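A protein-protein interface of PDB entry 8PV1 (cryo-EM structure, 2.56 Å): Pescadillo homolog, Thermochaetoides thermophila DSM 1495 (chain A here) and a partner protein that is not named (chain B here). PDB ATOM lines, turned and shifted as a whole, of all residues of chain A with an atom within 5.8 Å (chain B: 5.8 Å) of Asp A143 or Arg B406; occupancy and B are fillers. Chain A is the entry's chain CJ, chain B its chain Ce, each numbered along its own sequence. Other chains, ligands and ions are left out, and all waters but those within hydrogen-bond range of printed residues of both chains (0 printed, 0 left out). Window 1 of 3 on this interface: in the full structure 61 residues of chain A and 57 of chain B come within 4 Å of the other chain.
The side-chain amino group (NZ) of Lys B415 is in salt-bridge range of the side-chain carboxylate (OD2) of Asp A143 (3.5 Å). NH2 of Arg B413 is in salt-bridge range of OD2 of Asp A143 (2.5 Å). The side-chain carboxylate of Asp A143 is in salt-bridge range of the guanidinium group of Arg B406.
N of Leu A207 is in hydrogen-bond range of OD1 of Asp A142. O of Met B410 is in hydrogen-bond range of N of Lys B415 (3.1 Å). O of Asp A142 lies within hydrogen-bond range of OG of Ser A146 (3.1 Å). The guanidinium group (NH2) of Arg B413 is in hydrogen-bond range of the side-chain sulfur (SD) of Met B410. SG of Cys A144 lies within hydrogen-bond range of O of Tyr A234, at 3.3 Å. The side-chain hydroxyl (OH) of Tyr A234 sits at hydrogen-bond distance from the side-chain carboxylate (OD2) of Asp A143 (3.1 Å).
CE of Met B410 touches OD2 of Asp A143, 3.3 Å away. CG2 of Val B206 touches OG of Ser A146, at 3.4 Å. Arg B406 touches Ser A146. Leu A150 touches Leu B402 (CD2 to O, 3.7 Å). Arg B406 touches Leu A150 (CG to CD2, 3.8 Å). Leu A207 touches Val B206 (O to CG2, 3.5 Å). Tyr B407 touches Met A227. Met B410 touches Met A227. CE of Met B410 touches OH of Tyr A234 (3.9 Å). Lys B415 touches Tyr A234 (NZ to OH, 3.8 Å).
Printed residues of chain B within 4 Å of Leu A207: Val B206 (3.5 Å). Printed residues of chain A within 4 Å of Val B206: Ser A146 (3.4 Å) and Leu A207 (3.5 Å). Of chain A, only Asp A143, Ser A146 and Leu A150 come within 4 Å of Arg B406. Printed residues of chain A within 4 Å of Tyr B407: Met A227 (3.6 Å). Printed residues of chain A within 4 Å of Met B410: Asp A143, Met A227 and Tyr A234. Of the printed residues of chain A, Lys B415 touches Asp A143 and Tyr A234.
Of the 14 printed residues of chain A, 6 touch a printed residue of chain B. Of the 15 printed residues of chain B, 8 touch a printed residue of chain A. Hydrophobic or aromatic side chains of chain B within 4 Å of the printed part of chain A: Val B206, Leu B402, Leu B403, Tyr B407 and Met B410.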
ATOM      1  N   ARG A 139      -6.167  16.160 -17.292  1.00  0.00           N
ATOM      2  CA  ARG A 139      -6.388  15.812 -18.690  1.00  0.00           C
ATOM      3  C   ARG A 139      -5.164  16.038 -19.571  1.00  0.00           C
ATOM      4  O   ARG A 139      -5.033  15.360 -20.595  1.00  0.00           O
ATOM      5  CB  ARG A 139      -7.581  16.592 -19.246  1.00  0.00           C
ATOM      6  CG  ARG A 139      -8.901  16.219 -18.600  1.00  0.00           C
ATOM      7  CD  ARG A 139     -10.076  16.466 -19.526  1.00  0.00           C
ATOM      8  NE  ARG A 139     -11.292  16.780 -18.784  1.00  0.00           N
ATOM      9  CZ  ARG A 139     -11.563  17.963 -18.250  1.00  0.00           C
ATOM     10  NH1 ARG A 139     -10.738  18.989 -18.381  1.00  0.00           N
ATOM     11  NH2 ARG A 139     -12.695  18.123 -17.570  1.00  0.00           N
ATOM     12  N   ASP A 140      -4.273  16.964 -19.215  1.00  0.00           N
ATOM     13  CA  ASP A 140      -3.021  17.139 -19.951  1.00  0.00           C
ATOM     14  C   ASP A 140      -1.898  16.266 -19.382  1.00  0.00           C
ATOM     15  O   ASP A 140      -0.793  16.199 -19.959  1.00  0.00           O
ATOM     16  CB  ASP A 140      -2.628  18.619 -19.952  1.00  0.00           C
ATOM     17  CG  ASP A 140      -1.523  18.936 -20.941  1.00  0.00           C
ATOM     18  OD1 ASP A 140      -1.803  18.960 -22.159  1.00  0.00           O
ATOM     19  OD2 ASP A 140      -0.377  19.165 -20.502  1.00  0.00           O
ATOM     20  N   LEU A 141      -2.167  15.581 -18.266  1.00  0.00           N
ATOM     21  CA  LEU A 141      -1.190  14.672 -17.677  1.00  0.00           C
ATOM     22  C   LEU A 141      -0.766  13.536 -18.600  1.00  0.00           C
ATOM     23  O   LEU A 141       0.318  12.996 -18.398  1.00  0.00           O
ATOM     24  CB  LEU A 141      -1.724  14.078 -16.376  1.00  0.00           C
ATOM     25  CG  LEU A 141      -1.302  14.790 -15.092  1.00  0.00           C
ATOM     26  CD1 LEU A 141      -1.678  13.951 -13.888  1.00  0.00           C
ATOM     27  CD2 LEU A 141       0.188  15.081 -15.098  1.00  0.00           C
ATOM     28  N   ASP A 142      -1.572  13.162 -19.601  1.00  0.00           N
ATOM     29  CA  ASP A 142      -1.146  12.129 -20.548  1.00  0.00           C
ATOM     30  C   ASP A 142       0.107  12.558 -21.301  1.00  0.00           C
ATOM     31  O   ASP A 142       1.126  11.851 -21.301  1.00  0.00           O
ATOM     32  CB  ASP A 142      -2.271  11.830 -21.539  1.00  0.00           C
ATOM     33  CG  ASP A 142      -3.450  11.151 -20.893  1.00  0.00           C
ATOM     34  OD1 ASP A 142      -3.239  10.433 -19.901  1.00  0.00           O
ATOM     35  OD2 ASP A 142      -4.586  11.332 -21.377  1.00  0.00           O
ATOM     36  N   ASP A 143       0.053  13.739 -21.915  1.00  0.00           N
ATOM     37  CA  ASP A 143       1.201  14.283 -22.631  1.00  0.00           C
ATOM     38  C   ASP A 143       2.351  14.571 -21.678  1.00  0.00           C
ATOM     39  O   ASP A 143       3.518  14.298 -21.998  1.00  0.00           O
ATOM     40  CB  ASP A 143       0.782  15.547 -23.376  1.00  0.00           C
ATOM     41  CG  ASP A 143       1.562  15.758 -24.649  1.00  0.00           C
ATOM     42  OD1 ASP A 143       2.531  15.009 -24.891  1.00  0.00           O
ATOM     43  OD2 ASP A 143       1.192  16.670 -25.414  1.00  0.00           O
ATOM     44  N   CYS A 144       2.033  15.106 -20.489  1.00  0.00           N
ATOM     45  CA  CYS A 144       3.071  15.412 -19.505  1.00  0.00           C
ATOM     46  C   CYS A 144       3.842  14.163 -19.081  1.00  0.00           C
ATOM     47  O   CYS A 144       5.080  14.148 -19.083  1.00  0.00           O
ATOM     48  CB  CYS A 144       2.445  16.090 -18.285  1.00  0.00           C
ATOM     49  SG  CYS A 144       3.587  16.376 -16.916  1.00  0.00           S
ATOM     50  N   LEU A 145       3.118  13.091 -18.748  1.00  0.00           N
ATOM     51  CA  LEU A 145       3.750  11.866 -18.280  1.00  0.00           C
ATOM     52  C   LEU A 145       4.506  11.167 -19.395  1.00  0.00           C
ATOM     53  O   LEU A 145       5.591  10.628 -19.156  1.00  0.00           O
ATOM     54  CB  LEU A 145       2.704  10.929 -17.685  1.00  0.00           C
ATOM     55  CG  LEU A 145       2.140  11.307 -16.322  1.00  0.00           C
ATOM     56  CD1 LEU A 145       0.936  10.444 -16.037  1.00  0.00           C
ATOM     57  CD2 LEU A 145       3.190  11.154 -15.241  1.00  0.00           C
ATOM     58  N   SER A 146       3.955  11.156 -20.615  1.00  0.00           N
ATOM     59  CA  SER A 146       4.673  10.537 -21.724  1.00  0.00           C
ATOM     60  C   SER A 146       5.990  11.253 -21.994  1.00  0.00           C
ATOM     61  O   SER A 146       7.042  10.607 -22.105  1.00  0.00           O
ATOM     62  CB  SER A 146       3.798  10.522 -22.974  1.00  0.00           C
ATOM     63  OG  SER A 146       2.693   9.653 -22.802  1.00  0.00           O
ATOM     64  N   MET A 147       5.961  12.592 -22.021  1.00  0.00           N
ATOM     65  CA  MET A 147       7.173  13.368 -22.265  1.00  0.00           C
ATOM     66  C   MET A 147       8.204  13.163 -21.158  1.00  0.00           C
ATOM     67  O   MET A 147       9.390  12.943 -21.435  1.00  0.00           O
ATOM     68  CB  MET A 147       6.815  14.847 -22.395  1.00  0.00           C
ATOM     69  CG  MET A 147       7.974  15.744 -22.770  1.00  0.00           C
ATOM     70  SD  MET A 147       8.617  15.342 -24.401  1.00  0.00           S
ATOM     71  CE  MET A 147       7.293  15.978 -25.419  1.00  0.00           C
ATOM     72  N   LEU A 148       7.769  13.200 -19.895  1.00  0.00           N
ATOM     73  CA  LEU A 148       8.736  13.139 -18.802  1.00  0.00           C
ATOM     74  C   LEU A 148       9.284  11.730 -18.603  1.00  0.00           C
ATOM     75  O   LEU A 148      10.475  11.564 -18.315  1.00  0.00           O
ATOM     76  CB  LEU A 148       8.111  13.678 -17.517  1.00  0.00           C
ATOM     77  CG  LEU A 148       7.909  15.197 -17.525  1.00  0.00           C
ATOM     78  CD1 LEU A 148       7.509  15.695 -16.157  1.00  0.00           C
ATOM     79  CD2 LEU A 148       9.157  15.923 -18.006  1.00  0.00           C
ATOM     80  N   LEU A 150       9.636   9.634 -21.001  1.00  0.00           N
ATOM     81  CA  LEU A 150      10.574   9.486 -22.107  1.00  0.00           C
ATOM     82  C   LEU A 150      11.909  10.149 -21.792  1.00  0.00           C
ATOM     83  O   LEU A 150      12.975   9.560 -22.008  1.00  0.00           O
ATOM     84  CB  LEU A 150       9.962  10.074 -23.373  1.00  0.00           C
ATOM     85  CG  LEU A 150      10.838  10.145 -24.617  1.00  0.00           C
ATOM     86  CD1 LEU A 150      11.307   8.763 -25.029  1.00  0.00           C
ATOM     87  CD2 LEU A 150      10.050  10.806 -25.720  1.00  0.00           C
ATOM     88  N   LEU A 207      -3.750   7.846 -19.461  1.00  0.00           N
ATOM     89  CA  LEU A 207      -3.038   6.828 -20.222  1.00  0.00           C
ATOM     90  C   LEU A 207      -1.744   7.412 -20.765  1.00  0.00           C
ATOM     91  O   LEU A 207      -1.763   8.441 -21.446  1.00  0.00           O
ATOM     92  CB  LEU A 207      -3.905   6.307 -21.370  1.00  0.00           C
ATOM     93  CG  LEU A 207      -3.220   5.417 -22.406  1.00  0.00           C
ATOM     94  CD1 LEU A 207      -2.966   4.034 -21.844  1.00  0.00           C
ATOM     95  CD2 LEU A 207      -4.056   5.338 -23.669  1.00  0.00           C
ATOM     96  N   MET A 227      11.718  20.501 -27.786  1.00  0.00           N
ATOM     97  CA  MET A 227      11.282  19.388 -26.948  1.00  0.00           C
ATOM     98  C   MET A 227      11.722  19.589 -25.502  1.00  0.00           C
ATOM     99  O   MET A 227      10.977  19.278 -24.567  1.00  0.00           O
ATOM    100  CB  MET A 227      11.831  18.074 -27.501  1.00  0.00           C
ATOM    101  CG  MET A 227      11.017  17.475 -28.636  1.00  0.00           C
ATOM    102  SD  MET A 227       9.296  17.185 -28.204  1.00  0.00           S
ATOM    103  CE  MET A 227       8.461  18.195 -29.419  1.00  0.00           C
ATOM    104  N   TYR A 234       6.561  20.808 -18.627  1.00  0.00           N
ATOM    105  CA  TYR A 234       5.880  19.643 -18.086  1.00  0.00           C
ATOM    106  C   TYR A 234       6.374  19.283 -16.692  1.00  0.00           C
ATOM    107  O   TYR A 234       5.579  18.831 -15.864  1.00  0.00           O
ATOM    108  CB  TYR A 234       6.024  18.461 -19.041  1.00  0.00           C
ATOM    109  CG  TYR A 234       5.032  18.520 -20.175  1.00  0.00           C
ATOM    110  CD1 TYR A 234       3.746  18.995 -19.964  1.00  0.00           C
ATOM    111  CD2 TYR A 234       5.375  18.104 -21.453  1.00  0.00           C
ATOM    112  CE1 TYR A 234       2.831  19.057 -20.990  1.00  0.00           C
ATOM    113  CE2 TYR A 234       4.464  18.161 -22.489  1.00  0.00           C
ATOM    114  CZ  TYR A 234       3.193  18.639 -22.249  1.00  0.00           C
ATOM    115  OH  TYR A 234       2.279  18.700 -23.272  1.00  0.00           O
ATOM    116  N   ALA B 205      -3.513  12.858 -27.391  1.00  0.00           N
ATOM    117  CA  ALA B 205      -2.079  12.906 -27.126  1.00  0.00           C
ATOM    118  C   ALA B 205      -1.481  11.507 -27.087  1.00  0.00           C
ATOM    119  O   ALA B 205      -0.414  11.255 -27.659  1.00  0.00           O
ATOM    120  CB  ALA B 205      -1.814  13.645 -25.815  1.00  0.00           C
ATOM    121  N   VAL B 206      -2.154  10.582 -26.410  1.00  0.00           N
ATOM    122  CA  VAL B 206      -1.757   9.177 -26.392  1.00  0.00           C
ATOM    123  C   VAL B 206      -2.914   8.359 -26.953  1.00  0.00           C
ATOM    124  O   VAL B 206      -3.892   8.104 -26.234  1.00  0.00           O
ATOM    125  CB  VAL B 206      -1.376   8.714 -24.977  1.00  0.00           C
ATOM    126  CG1 VAL B 206      -0.950   7.256 -24.992  1.00  0.00           C
ATOM    127  CG2 VAL B 206      -0.269   9.582 -24.410  1.00  0.00           C
ATOM    128  N   ASN B 401      10.408   5.195 -32.701  1.00  0.00           N
ATOM    129  CA  ASN B 401      11.178   6.085 -31.843  1.00  0.00           C
ATOM    130  C   ASN B 401      10.182   6.976 -31.120  1.00  0.00           C
ATOM    131  O   ASN B 401       9.406   7.688 -31.764  1.00  0.00           O
ATOM    132  CB  ASN B 401      12.178   6.910 -32.660  1.00  0.00           C
ATOM    133  CG  ASN B 401      13.149   7.694 -31.795  1.00  0.00           C
ATOM    134  OD1 ASN B 401      13.083   7.660 -30.566  1.00  0.00           O
ATOM    135  ND2 ASN B 401      14.066   8.402 -32.440  1.00  0.00           N
ATOM    136  N   LEU B 402      10.197   6.930 -29.787  1.00  0.00           N
ATOM    137  CA  LEU B 402       9.161   7.615 -29.022  1.00  0.00           C
ATOM    138  C   LEU B 402       9.358   9.125 -29.030  1.00  0.00           C
ATOM    139  O   LEU B 402       8.383   9.877 -28.942  1.00  0.00           O
ATOM    140  CB  LEU B 402       9.117   7.076 -27.593  1.00  0.00           C
ATOM    141  CG  LEU B 402       8.612   5.637 -27.446  1.00  0.00           C
ATOM    142  CD1 LEU B 402       8.284   5.336 -26.003  1.00  0.00           C
ATOM    143  CD2 LEU B 402       7.400   5.383 -28.326  1.00  0.00           C
ATOM    144  N   LEU B 403      10.604   9.590 -29.143  1.00  0.00           N
ATOM    145  CA  LEU B 403      10.842  11.025 -29.284  1.00  0.00           C
ATOM    146  C   LEU B 403      10.277  11.548 -30.599  1.00  0.00           C
ATOM    147  O   LEU B 403       9.638  12.611 -30.638  1.00  0.00           O
ATOM    148  CB  LEU B 403      12.339  11.313 -29.180  1.00  0.00           C
ATOM    149  CG  LEU B 403      12.752  12.781 -29.101  1.00  0.00           C
ATOM    150  CD1 LEU B 403      12.056  13.463 -27.937  1.00  0.00           C
ATOM    151  CD2 LEU B 403      14.258  12.898 -28.969  1.00  0.00           C
ATOM    152  N   LYS B 404      10.483  10.795 -31.683  1.00  0.00           N
ATOM    153  CA  LYS B 404       9.873  11.133 -32.964  1.00  0.00           C
ATOM    154  C   LYS B 404       8.355  11.069 -32.882  1.00  0.00           C
ATOM    155  O   LYS B 404       7.658  11.882 -33.497  1.00  0.00           O
ATOM    156  CB  LYS B 404      10.390  10.193 -34.051  1.00  0.00           C
ATOM    157  CG  LYS B 404       9.923  10.538 -35.452  1.00  0.00           C
ATOM    158  CD  LYS B 404      10.344   9.474 -36.449  1.00  0.00           C
ATOM    159  CE  LYS B 404      11.832   9.537 -36.729  1.00  0.00           C
ATOM    160  NZ  LYS B 404      12.182  10.759 -37.497  1.00  0.00           N
ATOM    161  N   ASP B 405       7.827  10.109 -32.116  1.00  0.00           N
ATOM    162  CA  ASP B 405       6.383   9.996 -31.946  1.00  0.00           C
ATOM    163  C   ASP B 405       5.807  11.207 -31.223  1.00  0.00           C
ATOM    164  O   ASP B 405       4.756  11.725 -31.613  1.00  0.00           O
ATOM    165  CB  ASP B 405       6.046   8.711 -31.194  1.00  0.00           C
ATOM    166  CG  ASP B 405       5.843   7.534 -32.121  1.00  0.00           C
ATOM    167  OD1 ASP B 405       5.503   6.440 -31.629  1.00  0.00           O
ATOM    168  OD2 ASP B 405       6.025   7.704 -33.344  1.00  0.00           O
ATOM    169  N   ARG B 406       6.485  11.676 -30.171  1.00  0.00           N
ATOM    170  CA  ARG B 406       6.011  12.853 -29.446  1.00  0.00           C
ATOM    171  C   ARG B 406       6.108  14.109 -30.302  1.00  0.00           C
ATOM    172  O   ARG B 406       5.214  14.965 -30.262  1.00  0.00           O
ATOM    173  CB  ARG B 406       6.795  13.034 -28.145  1.00  0.00           C
ATOM    174  CG  ARG B 406       6.654  11.894 -27.148  1.00  0.00           C
ATOM    175  CD  ARG B 406       5.655  12.189 -26.037  1.00  0.00           C
ATOM    176  NE  ARG B 406       4.364  12.655 -26.529  1.00  0.00           N
ATOM    177  CZ  ARG B 406       3.415  11.865 -27.010  1.00  0.00           C
ATOM    178  NH1 ARG B 406       3.583  10.556 -27.098  1.00  0.00           N
ATOM    179  NH2 ARG B 406       2.265  12.399 -27.408  1.00  0.00           N
ATOM    180  N   TYR B 407       7.182  14.234 -31.088  1.00  0.00           N
ATOM    181  CA  TYR B 407       7.314  15.379 -31.986  1.00  0.00           C
ATOM    182  C   TYR B 407       6.227  15.377 -33.061  1.00  0.00           C
ATOM    183  O   TYR B 407       5.620  16.420 -33.350  1.00  0.00           O
ATOM    184  CB  TYR B 407       8.707  15.375 -32.611  1.00  0.00           C
ATOM    185  CG  TYR B 407       9.008  16.558 -33.498  1.00  0.00           C
ATOM    186  CD1 TYR B 407       8.910  17.854 -33.017  1.00  0.00           C
ATOM    187  CD2 TYR B 407       9.415  16.375 -34.813  1.00  0.00           C
ATOM    188  CE1 TYR B 407       9.191  18.938 -33.824  1.00  0.00           C
ATOM    189  CE2 TYR B 407       9.701  17.451 -35.627  1.00  0.00           C
ATOM    190  CZ  TYR B 407       9.587  18.730 -35.128  1.00  0.00           C
ATOM    191  OH  TYR B 407       9.868  19.806 -35.935  1.00  0.00           O
ATOM    192  N   ARG B 408       5.952  14.206 -33.646  1.00  0.00           N
ATOM    193  CA  ARG B 408       4.893  14.104 -34.644  1.00  0.00           C
ATOM    194  C   ARG B 408       3.525  14.361 -34.032  1.00  0.00           C
ATOM    195  O   ARG B 408       2.655  14.947 -34.679  1.00  0.00           O
ATOM    196  CB  ARG B 408       4.918  12.733 -35.315  1.00  0.00           C
ATOM    197  CG  ARG B 408       5.865  12.623 -36.489  1.00  0.00           C
ATOM    198  CD  ARG B 408       5.675  11.296 -37.199  1.00  0.00           C
ATOM    199  NE  ARG B 408       4.289  11.103 -37.608  1.00  0.00           N
ATOM    200  CZ  ARG B 408       3.854  11.215 -38.856  1.00  0.00           C
ATOM    201  NH1 ARG B 408       4.675  11.507 -39.851  1.00  0.00           N
ATOM    202  NH2 ARG B 408       2.563  11.026 -39.113  1.00  0.00           N
ATOM    203  N   SER B 409       3.312  13.919 -32.790  1.00  0.00           N
ATOM    204  CA  SER B 409       2.057  14.208 -32.106  1.00  0.00           C
ATOM    205  C   SER B 409       1.892  15.702 -31.873  1.00  0.00           C
ATOM    206  O   SER B 409       0.789  16.241 -32.026  1.00  0.00           O
ATOM    207  CB  SER B 409       1.992  13.448 -30.784  1.00  0.00           C
ATOM    208  OG  SER B 409       0.783  13.723 -30.100  1.00  0.00           O
ATOM    209  N   MET B 410       2.986  16.383 -31.515  1.00  0.00           N
ATOM    210  CA  MET B 410       2.956  17.832 -31.340  1.00  0.00           C
ATOM    211  C   MET B 410       2.561  18.532 -32.635  1.00  0.00           C
ATOM    212  O   MET B 410       1.702  19.423 -32.637  1.00  0.00           O
ATOM    213  CB  MET B 410       4.330  18.325 -30.887  1.00  0.00           C
ATOM    214  CG  MET B 410       4.609  18.224 -29.400  1.00  0.00           C
ATOM    215  SD  MET B 410       3.251  18.686 -28.323  1.00  0.00           S
ATOM    216  CE  MET B 410       3.835  17.988 -26.783  1.00  0.00           C
ATOM    217  N   ILE B 411       3.160  18.114 -33.754  1.00  0.00           N
ATOM    218  CA  ILE B 411       2.862  18.747 -35.039  1.00  0.00           C
ATOM    219  C   ILE B 411       1.433  18.441 -35.481  1.00  0.00           C
ATOM    220  O   ILE B 411       0.710  19.329 -35.946  1.00  0.00           O
ATOM    221  CB  ILE B 411       3.887  18.319 -36.104  1.00  0.00           C
ATOM    222  CG1 ILE B 411       5.298  18.697 -35.665  1.00  0.00           C
ATOM    223  CG2 ILE B 411       3.574  18.969 -37.441  1.00  0.00           C
ATOM    224  CD1 ILE B 411       6.361  18.264 -36.634  1.00  0.00           C
ATOM    225  N   ARG B 413      -1.256  17.539 -33.661  1.00  0.00           N
ATOM    226  CA  ARG B 413      -2.189  18.296 -32.841  1.00  0.00           C
ATOM    227  C   ARG B 413      -2.044  19.801 -33.021  1.00  0.00           C
ATOM    228  O   ARG B 413      -2.933  20.546 -32.601  1.00  0.00           O
ATOM    229  CB  ARG B 413      -2.024  17.924 -31.368  1.00  0.00           C
ATOM    230  CG  ARG B 413      -2.573  16.551 -31.033  1.00  0.00           C
ATOM    231  CD  ARG B 413      -2.394  16.238 -29.567  1.00  0.00           C
ATOM    232  NE  ARG B 413      -0.992  16.034 -29.230  1.00  0.00           N
ATOM    233  CZ  ARG B 413      -0.453  16.342 -28.060  1.00  0.00           C
ATOM    234  NH1 ARG B 413      -1.172  16.880 -27.090  1.00  0.00           N
ATOM    235  NH2 ARG B 413       0.839  16.105 -27.859  1.00  0.00           N
ATOM    236  N   LYS B 415       0.344  22.185 -32.066  1.00  0.00           N
ATOM    237  CA  LYS B 415       0.956  23.122 -31.136  1.00  0.00           C
ATOM    238  C   LYS B 415       2.163  23.817 -31.750  1.00  0.00           C
ATOM    239  O   LYS B 415       2.557  24.892 -31.286  1.00  0.00           O
ATOM    240  CB  LYS B 415       1.342  22.399 -29.847  1.00  0.00           C
ATOM    241  CG  LYS B 415       0.156  21.771 -29.137  1.00  0.00           C
ATOM    242  CD  LYS B 415       0.573  21.081 -27.857  1.00  0.00           C
ATOM    243  CE  LYS B 415      -0.632  20.562 -27.095  1.00  0.00           C
ATOM    244  NZ  LYS B 415      -0.231  19.889 -25.830  1.00  0.00           N
